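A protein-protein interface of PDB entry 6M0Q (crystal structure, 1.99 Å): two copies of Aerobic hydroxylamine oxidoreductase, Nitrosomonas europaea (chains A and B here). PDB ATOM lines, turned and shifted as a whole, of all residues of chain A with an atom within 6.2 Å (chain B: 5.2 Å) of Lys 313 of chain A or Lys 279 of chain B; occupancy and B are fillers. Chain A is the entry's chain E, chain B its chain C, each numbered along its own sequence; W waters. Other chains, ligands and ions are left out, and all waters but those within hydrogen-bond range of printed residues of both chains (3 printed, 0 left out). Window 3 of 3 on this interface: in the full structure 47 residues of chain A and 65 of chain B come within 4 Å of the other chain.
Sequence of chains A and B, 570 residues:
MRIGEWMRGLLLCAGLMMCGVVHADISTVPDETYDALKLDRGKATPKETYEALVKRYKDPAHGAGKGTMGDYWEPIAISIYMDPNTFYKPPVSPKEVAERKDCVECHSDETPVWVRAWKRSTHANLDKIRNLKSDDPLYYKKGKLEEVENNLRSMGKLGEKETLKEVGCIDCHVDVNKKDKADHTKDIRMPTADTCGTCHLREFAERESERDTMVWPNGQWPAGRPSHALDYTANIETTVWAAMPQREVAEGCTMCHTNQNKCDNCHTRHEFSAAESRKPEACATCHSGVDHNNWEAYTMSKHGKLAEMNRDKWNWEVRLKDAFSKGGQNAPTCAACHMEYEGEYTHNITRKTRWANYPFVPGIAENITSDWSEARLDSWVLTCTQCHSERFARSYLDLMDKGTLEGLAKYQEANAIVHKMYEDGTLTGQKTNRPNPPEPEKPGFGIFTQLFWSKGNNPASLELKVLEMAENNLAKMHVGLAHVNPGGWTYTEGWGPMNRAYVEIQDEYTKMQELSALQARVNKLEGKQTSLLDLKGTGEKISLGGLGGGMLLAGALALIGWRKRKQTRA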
ATOM      1  N   GLU A 308     -14.844 -18.576  21.866  1.00  0.00           N
ATOM      2  CA  GLU A 308     -13.444 -18.959  22.097  1.00  0.00           C
ATOM      3  C   GLU A 308     -13.374 -20.224  22.923  1.00  0.00           C
ATOM      4  O   GLU A 308     -12.752 -21.198  22.513  1.00  0.00           O
ATOM      5  CB  GLU A 308     -12.646 -17.836  22.782  1.00  0.00           C
ATOM      6  CG  GLU A 308     -12.048 -16.838  21.776  1.00  0.00           C
ATOM      7  CD  GLU A 308     -11.724 -15.427  22.345  1.00  0.00           C
ATOM      8  OE1 GLU A 308     -11.362 -15.258  23.567  1.00  0.00           O
ATOM      9  OE2 GLU A 308     -11.832 -14.478  21.518  1.00  0.00           O
ATOM     10  N   MET A 309     -14.099 -20.259  24.042  1.00  0.00           N
ATOM     11  CA  MET A 309     -14.052 -21.407  24.940  1.00  0.00           C
ATOM     12  C   MET A 309     -14.592 -22.677  24.307  1.00  0.00           C
ATOM     13  O   MET A 309     -14.158 -23.772  24.674  1.00  0.00           O
ATOM     14  CB  MET A 309     -14.853 -21.107  26.208  1.00  0.00           C
ATOM     15  CG  MET A 309     -14.160 -20.104  27.062  1.00  0.00           C
ATOM     16  SD  MET A 309     -15.026 -19.858  28.629  1.00  0.00           S
ATOM     17  CE  MET A 309     -16.283 -18.702  28.111  1.00  0.00           C
ATOM     18  N   ASN A 310     -15.564 -22.571  23.408  1.00  0.00           N
ATOM     19  CA  ASN A 310     -16.243 -23.749  22.888  1.00  0.00           C
ATOM     20  C   ASN A 310     -15.844 -24.092  21.461  1.00  0.00           C
ATOM     21  O   ASN A 310     -16.443 -24.983  20.862  1.00  0.00           O
ATOM     22  CB  ASN A 310     -17.760 -23.559  22.974  1.00  0.00           C
ATOM     23  CG  ASN A 310     -18.255 -23.590  24.383  1.00  0.00           C
ATOM     24  OD1 ASN A 310     -17.725 -24.313  25.201  1.00  0.00           O
ATOM     25  ND2 ASN A 310     -19.271 -22.804  24.683  1.00  0.00           N
ATOM     26  N   ARG A 311     -14.826 -23.435  20.915  1.00  0.00           N
ATOM     27  CA  ARG A 311     -14.564 -23.582  19.490  1.00  0.00           C
ATOM     28  C   ARG A 311     -14.215 -25.015  19.132  1.00  0.00           C
ATOM     29  O   ARG A 311     -14.536 -25.473  18.033  1.00  0.00           O
ATOM     30  CB  ARG A 311     -13.445 -22.646  19.069  1.00  0.00           C
ATOM     31  CG  ARG A 311     -12.185 -22.873  19.833  1.00  0.00           C
ATOM     32  CD  ARG A 311     -10.989 -22.408  19.044  1.00  0.00           C
ATOM     33  NE  ARG A 311     -10.977 -20.967  18.786  1.00  0.00           N
ATOM     34  CZ  ARG A 311     -10.449 -20.059  19.605  1.00  0.00           C
ATOM     35  NH1 ARG A 311      -9.893 -20.439  20.751  1.00  0.00           N
ATOM     36  NH2 ARG A 311     -10.485 -18.767  19.278  1.00  0.00           N
ATOM     37  N   ASP A 312     -13.585 -25.751  20.045  1.00  0.00           N
ATOM     38  CA  ASP A 312     -13.179 -27.117  19.735  1.00  0.00           C
ATOM     39  C   ASP A 312     -14.277 -28.144  19.991  1.00  0.00           C
ATOM     40  O   ASP A 312     -14.090 -29.320  19.659  1.00  0.00           O
ATOM     41  CB  ASP A 312     -11.901 -27.469  20.511  1.00  0.00           C
ATOM     42  CG  ASP A 312     -10.668 -26.677  20.002  1.00  0.00           C
ATOM     43  OD1 ASP A 312     -10.749 -26.094  18.886  1.00  0.00           O
ATOM     44  OD2 ASP A 312      -9.623 -26.639  20.706  1.00  0.00           O
ATOM     45  N   LYS A 313     -15.415 -27.738  20.554  1.00  0.00           N
ATOM     46  CA  LYS A 313     -16.577 -28.608  20.628  1.00  0.00           C
ATOM     47  C   LYS A 313     -17.453 -28.517  19.387  1.00  0.00           C
ATOM     48  O   LYS A 313     -18.259 -29.417  19.137  1.00  0.00           O
ATOM     49  CB  LYS A 313     -17.425 -28.266  21.859  1.00  0.00           C
ATOM     50  CG  LYS A 313     -16.665 -28.272  23.157  1.00  0.00           C
ATOM     51  CD  LYS A 313     -17.600 -28.032  24.339  1.00  0.00           C
ATOM     52  CE  LYS A 313     -16.823 -27.944  25.656  1.00  0.00           C
ATOM     53  NZ  LYS A 313     -15.746 -26.897  25.565  1.00  0.00           N
ATOM     54  N   TRP A 314     -17.310 -27.466  18.605  1.00  0.00           N
ATOM     55  CA  TRP A 314     -18.206 -27.218  17.488  1.00  0.00           C
ATOM     56  C   TRP A 314     -17.704 -27.915  16.223  1.00  0.00           C
ATOM     57  O   TRP A 314     -16.502 -28.062  16.004  1.00  0.00           O
ATOM     58  CB  TRP A 314     -18.334 -25.717  17.247  1.00  0.00           C
ATOM     59  CG  TRP A 314     -18.903 -24.960  18.393  1.00  0.00           C
ATOM     60  CD1 TRP A 314     -19.429 -25.474  19.554  1.00  0.00           C
ATOM     61  CD2 TRP A 314     -19.012 -23.538  18.495  1.00  0.00           C
ATOM     62  NE1 TRP A 314     -19.854 -24.451  20.370  1.00  0.00           N
ATOM     63  CE2 TRP A 314     -19.621 -23.252  19.736  1.00  0.00           C
ATOM     64  CE3 TRP A 314     -18.666 -22.476  17.648  1.00  0.00           C
ATOM     65  CZ2 TRP A 314     -19.887 -21.943  20.156  1.00  0.00           C
ATOM     66  CZ3 TRP A 314     -18.924 -21.173  18.071  1.00  0.00           C
ATOM     67  CH2 TRP A 314     -19.536 -20.922  19.312  1.00  0.00           C
ATOM     68  N   ASN A 315     -18.644 -28.380  15.411  1.00  0.00           N
ATOM     69  CA  ASN A 315     -18.318 -28.914  14.096  1.00  0.00           C
ATOM     70  C   ASN A 315     -18.487 -27.783  13.103  1.00  0.00           C
ATOM     71  O   ASN A 315     -19.597 -27.507  12.613  1.00  0.00           O
ATOM     72  CB  ASN A 315     -19.188 -30.106  13.740  1.00  0.00           C
ATOM     73  CG  ASN A 315     -18.789 -30.711  12.427  1.00  0.00           C
ATOM     74  OD1 ASN A 315     -17.884 -30.203  11.745  1.00  0.00           O
ATOM     75  ND2 ASN A 315     -19.456 -31.794  12.050  1.00  0.00           N
ATOM     76  N   GLY A 327     -24.127 -28.806  14.427  1.00  0.00           N
ATOM     77  CA  GLY A 327     -22.754 -28.426  14.713  1.00  0.00           C
ATOM     78  C   GLY A 327     -22.429 -28.302  16.187  1.00  0.00           C
ATOM     79  O   GLY A 327     -21.272 -28.056  16.542  1.00  0.00           O
ATOM     80  N   GLY A 328     -23.433 -28.444  17.047  1.00  0.00           N
ATOM     81  CA  GLY A 328     -23.277 -28.231  18.469  1.00  0.00           C
ATOM     82  C   GLY A 328     -22.952 -26.804  18.871  1.00  0.00           C
ATOM     83  O   GLY A 328     -22.580 -26.560  20.025  1.00  0.00           O
ATOM     84  N   GLN A 329     -23.093 -25.847  17.951  1.00  0.00           N
ATOM     85  CA  GLN A 329     -22.771 -24.463  18.269  1.00  0.00           C
ATOM     86  C   GLN A 329     -23.833 -23.865  19.184  1.00  0.00           C
ATOM     87  O   GLN A 329     -25.033 -24.005  18.935  1.00  0.00           O
ATOM     88  CB  GLN A 329     -22.649 -23.634  16.991  1.00  0.00           C
ATOM     89  CG  GLN A 329     -22.114 -22.240  17.263  1.00  0.00           C
ATOM     90  CD  GLN A 329     -21.896 -21.435  16.030  1.00  0.00           C
ATOM     91  OE1 GLN A 329     -21.617 -21.982  14.953  1.00  0.00           O
ATOM     92  NE2 GLN A 329     -22.016 -20.111  16.165  1.00  0.00           N
ATOM     93  N   ALA B 275     -16.649 -26.539  33.651  1.00  0.00           N
ATOM     94  CA  ALA B 275     -15.438 -26.459  32.824  1.00  0.00           C
ATOM     95  C   ALA B 275     -15.310 -25.090  32.167  1.00  0.00           C
ATOM     96  O   ALA B 275     -14.208 -24.537  32.056  1.00  0.00           O
ATOM     97  CB  ALA B 275     -15.443 -27.548  31.746  1.00  0.00           C
ATOM     98  N   GLU B 276     -16.430 -24.534  31.704  1.00  0.00           N
ATOM     99  CA  GLU B 276     -16.402 -23.208  31.111  1.00  0.00           C
ATOM    100  C   GLU B 276     -15.962 -22.162  32.124  1.00  0.00           C
ATOM    101  O   GLU B 276     -15.081 -21.345  31.843  1.00  0.00           O
ATOM    102  CB  GLU B 276     -17.785 -22.872  30.555  1.00  0.00           C
ATOM    103  CG  GLU B 276     -17.932 -21.442  30.067  1.00  0.00           C
ATOM    104  CD  GLU B 276     -19.403 -21.104  29.766  1.00  0.00           C
ATOM    105  OE1 GLU B 276     -20.094 -21.960  29.180  1.00  0.00           O
ATOM    106  OE2 GLU B 276     -19.866 -20.009  30.145  1.00  0.00           O
ATOM    107  N   SER B 277     -16.572 -22.168  33.314  1.00  0.00           N
ATOM    108  CA  SER B 277     -16.270 -21.155  34.311  1.00  0.00           C
ATOM    109  C   SER B 277     -14.849 -21.265  34.856  1.00  0.00           C
ATOM    110  O   SER B 277     -14.351 -20.294  35.419  1.00  0.00           O
ATOM    111  CB  SER B 277     -17.286 -21.234  35.455  1.00  0.00           C
ATOM    112  OG  SER B 277     -17.245 -22.522  36.002  1.00  0.00           O
ATOM    113  N   ARG B 278     -14.185 -22.410  34.702  1.00  0.00           N
ATOM    114  CA  ARG B 278     -12.759 -22.525  35.036  1.00  0.00           C
ATOM    115  C   ARG B 278     -11.851 -21.895  33.990  1.00  0.00           C
ATOM    116  O   ARG B 278     -10.672 -21.625  34.269  1.00  0.00           O
ATOM    117  CB  ARG B 278     -12.381 -24.001  35.212  1.00  0.00           C
ATOM    118  CG  ARG B 278     -13.147 -24.656  36.351  1.00  0.00           C
ATOM    119  CD  ARG B 278     -12.762 -26.124  36.529  1.00  0.00           C
ATOM    120  NE  ARG B 278     -13.595 -26.723  37.554  1.00  0.00           N
ATOM    121  CZ  ARG B 278     -14.500 -27.662  37.340  1.00  0.00           C
ATOM    122  NH1 ARG B 278     -14.675 -28.144  36.127  1.00  0.00           N
ATOM    123  NH2 ARG B 278     -15.246 -28.113  38.348  1.00  0.00           N
ATOM    124  N   LYS B 279     -12.358 -21.658  32.821  1.00  0.00           N
ATOM    125  CA  LYS B 279     -11.496 -21.079  31.800  1.00  0.00           C
ATOM    126  C   LYS B 279     -11.337 -19.585  32.033  1.00  0.00           C
ATOM    127  O   LYS B 279     -12.305 -18.906  32.393  1.00  0.00           O
ATOM    128  CB  LYS B 279     -12.075 -21.320  30.418  1.00  0.00           C
ATOM    129  CG  LYS B 279     -12.117 -22.792  30.105  1.00  0.00           C
ATOM    130  CD  LYS B 279     -12.712 -23.079  28.744  1.00  0.00           C
ATOM    131  CE  LYS B 279     -12.798 -24.592  28.526  1.00  0.00           C
ATOM    132  NZ  LYS B 279     -13.209 -24.913  27.139  1.00  0.00           N
ATOM    133  N   PRO B 280     -10.141 -19.046  31.809  1.00  0.00           N
ATOM    134  CA  PRO B 280      -9.938 -17.600  32.008  1.00  0.00           C
ATOM    135  C   PRO B 280     -10.908 -16.742  31.219  1.00  0.00           C
ATOM    136  O   PRO B 280     -11.314 -15.670  31.686  1.00  0.00           O
ATOM    137  CB  PRO B 280      -8.493 -17.379  31.541  1.00  0.00           C
ATOM    138  CG  PRO B 280      -7.830 -18.756  31.649  1.00  0.00           C
ATOM    139  CD  PRO B 280      -8.924 -19.758  31.379  1.00  0.00           C
ATOM    140  N   GLU B 281     -11.289 -17.185  30.027  1.00  0.00           N
ATOM    141  CA  GLU B 281     -12.237 -16.427  29.210  1.00  0.00           C
ATOM    142  C   GLU B 281     -13.525 -16.093  29.962  1.00  0.00           C
ATOM    143  O   GLU B 281     -14.169 -15.072  29.682  1.00  0.00           O
ATOM    144  CB  GLU B 281     -12.566 -17.224  27.951  1.00  0.00           C
ATOM    145  CG  GLU B 281     -11.457 -17.238  26.900  1.00  0.00           C
ATOM    146  CD  GLU B 281     -10.302 -18.221  27.178  1.00  0.00           C
ATOM    147  OE1 GLU B 281     -10.323 -18.990  28.176  1.00  0.00           O
ATOM    148  OE2 GLU B 281      -9.353 -18.196  26.362  1.00  0.00           O
ATOM    149  N   ALA B 282     -13.924 -16.945  30.900  1.00  0.00           N
ATOM    150  CA  ALA B 282     -15.143 -16.712  31.667  1.00  0.00           C
ATOM    151  C   ALA B 282     -15.118 -15.390  32.405  1.00  0.00           C
ATOM    152  O   ALA B 282     -16.176 -14.785  32.615  1.00  0.00           O
ATOM    153  CB  ALA B 282     -15.356 -17.844  32.672  1.00  0.00           C
ATOM    154  N   CYS B 283     -13.939 -14.943  32.832  1.00  0.00           N
ATOM    155  CA  CYS B 283     -13.806 -13.736  33.632  1.00  0.00           C
ATOM    156  C   CYS B 283     -13.610 -12.516  32.772  1.00  0.00           C
ATOM    157  O   CYS B 283     -13.672 -11.394  33.284  1.00  0.00           O
ATOM    158  CB  CYS B 283     -12.604 -13.845  34.582  1.00  0.00           C
ATOM    159  SG  CYS B 283     -12.344 -15.450  35.321  1.00  0.00           S
ATOM    160  N   TRP B 316     -10.485 -29.630  31.482  1.00  0.00           N
ATOM    161  CA  TRP B 316     -11.133 -28.544  32.207  1.00  0.00           C
ATOM    162  C   TRP B 316     -12.305 -29.014  33.065  1.00  0.00           C
ATOM    163  O   TRP B 316     -12.815 -28.233  33.869  1.00  0.00           O
ATOM    164  CB  TRP B 316     -11.613 -27.492  31.215  1.00  0.00           C
ATOM    165  CG  TRP B 316     -10.533 -26.758  30.497  1.00  0.00           C
ATOM    166  CD1 TRP B 316     -10.070 -27.013  29.233  1.00  0.00           C
ATOM    167  CD2 TRP B 316      -9.817 -25.603  30.959  1.00  0.00           C
ATOM    168  NE1 TRP B 316      -9.092 -26.111  28.905  1.00  0.00           N
ATOM    169  CE2 TRP B 316      -8.935 -25.223  29.936  1.00  0.00           C
ATOM    170  CE3 TRP B 316      -9.856 -24.844  32.130  1.00  0.00           C
ATOM    171  CZ2 TRP B 316      -8.085 -24.133  30.049  1.00  0.00           C
ATOM    172  CZ3 TRP B 316      -9.007 -23.773  32.246  1.00  0.00           C
ATOM    173  CH2 TRP B 316      -8.137 -23.418  31.209  1.00  0.00           C
HETATM  174  O   HOH W   1      -9.137 -16.720  24.359  1.00  0.00           O
HETATM  175  O   HOH W   2     -15.978 -24.435  27.766  1.00  0.00           O
HETATM  176  O   HOH W   3     -21.656 -22.804  26.897  1.00  0.00           O
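NZ of Lys 279 of chain B is in hydrogen-bond range of O of Met 309 of chain A, 2.9 Å away. O of Glu 276 of chain B lies close to SD of Met 309 of chain A (3.5 Å).
The backbone carbonyl oxygen (O) of Glu 308 of chain A sits close to the guanidinium group (NH1) of Arg 311 of chain A, 3.4 Å away. The side-chain amide oxygen (OD1) of Asn 310 of chain A lies within hydrogen-bond range of the side-chain amino group (NZ) of Lys 313 of chain A, 3.3 Å away.
OE1 of Glu 308 of chain A touches CG of Glu 281 of chain B, 3.9 Å away. Met 309 of chain A touches Glu 281 of chain B. N of Ala 282 of chain B touches SD of Met 309 of chain A (3.9 Å). Lys 313 of chain A touches Lys 279 of chain B.
Lys 313 of chain A touches one residue of chain B. Lys 279 of chain B touches just these residues of chain A: Met 309 and Lys 313. Printed residues of chain B within 4 Å of Met 309 of chain A: Glu 276 (3.5 Å), Lys 279 (2.9 Å), Glu 281 (3.4 Å) and Ala 282 (3.9 Å). Of the printed residues of chain B, Glu 308 of chain A touches Glu 281. Of the printed residues of chain A, Glu 276 of chain B touches Met 309. Printed residues of chain A within 4 Å of Glu 281 of chain B: Glu 308 (3.9 Å) and Met 309 (3.4 Å). Of the printed residues of chain A, Ala 282 of chain B touches Met 309. Gln 329 of chain A touches none of the printed residues of chain B. Arg 278 of chain B touches none of the printed residues of chain A. The nearest printed residue of chain B that does not touch Lys 313 of chain A is Ala 275 of chain B (6.2 Å). The nearest residue of chain A that does not touch Lys 279 of chain B is Asn 310 of chain A (5.0 Å).
Of the 11 printed residues of chain A, 3 touch a printed residue of chain B. Printed residues of chain A that touch a printed residue of chain B: Glu 308, Met 309 and Lys 313. Among the printed residues, 6 pairs touch across the chains. Among the printed residues, no Asp or Glu carboxylate lies within 4 Å of a Lys or Arg side-chain nitrogen of the other chain.
No position is printed for both chains. Of the 6 pairs that touch across the chains among the printed residues, none has its exchanged pair printed and touching as well.
Water W1 lies within hydrogen-bond range of the side-chain carboxylate of Glu 281 of chain B (2.5 Å) and the side-chain carboxylate of Glu 308 of chain A (2.8 Å). Water W2 lies within hydrogen-bond range of NZ of Lys 279 of chain B (2.9 Å), OD1 of Asn 310 of chain A (3.1 Å) and NZ of Lys 313 of chain A (3.3 Å). Water W3 bridges the side-chain carboxylate of Glu 276 of chain B (2.9 Å) and the side-chain amide nitrogen of Asn 310 of chain A (3.3 Å).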
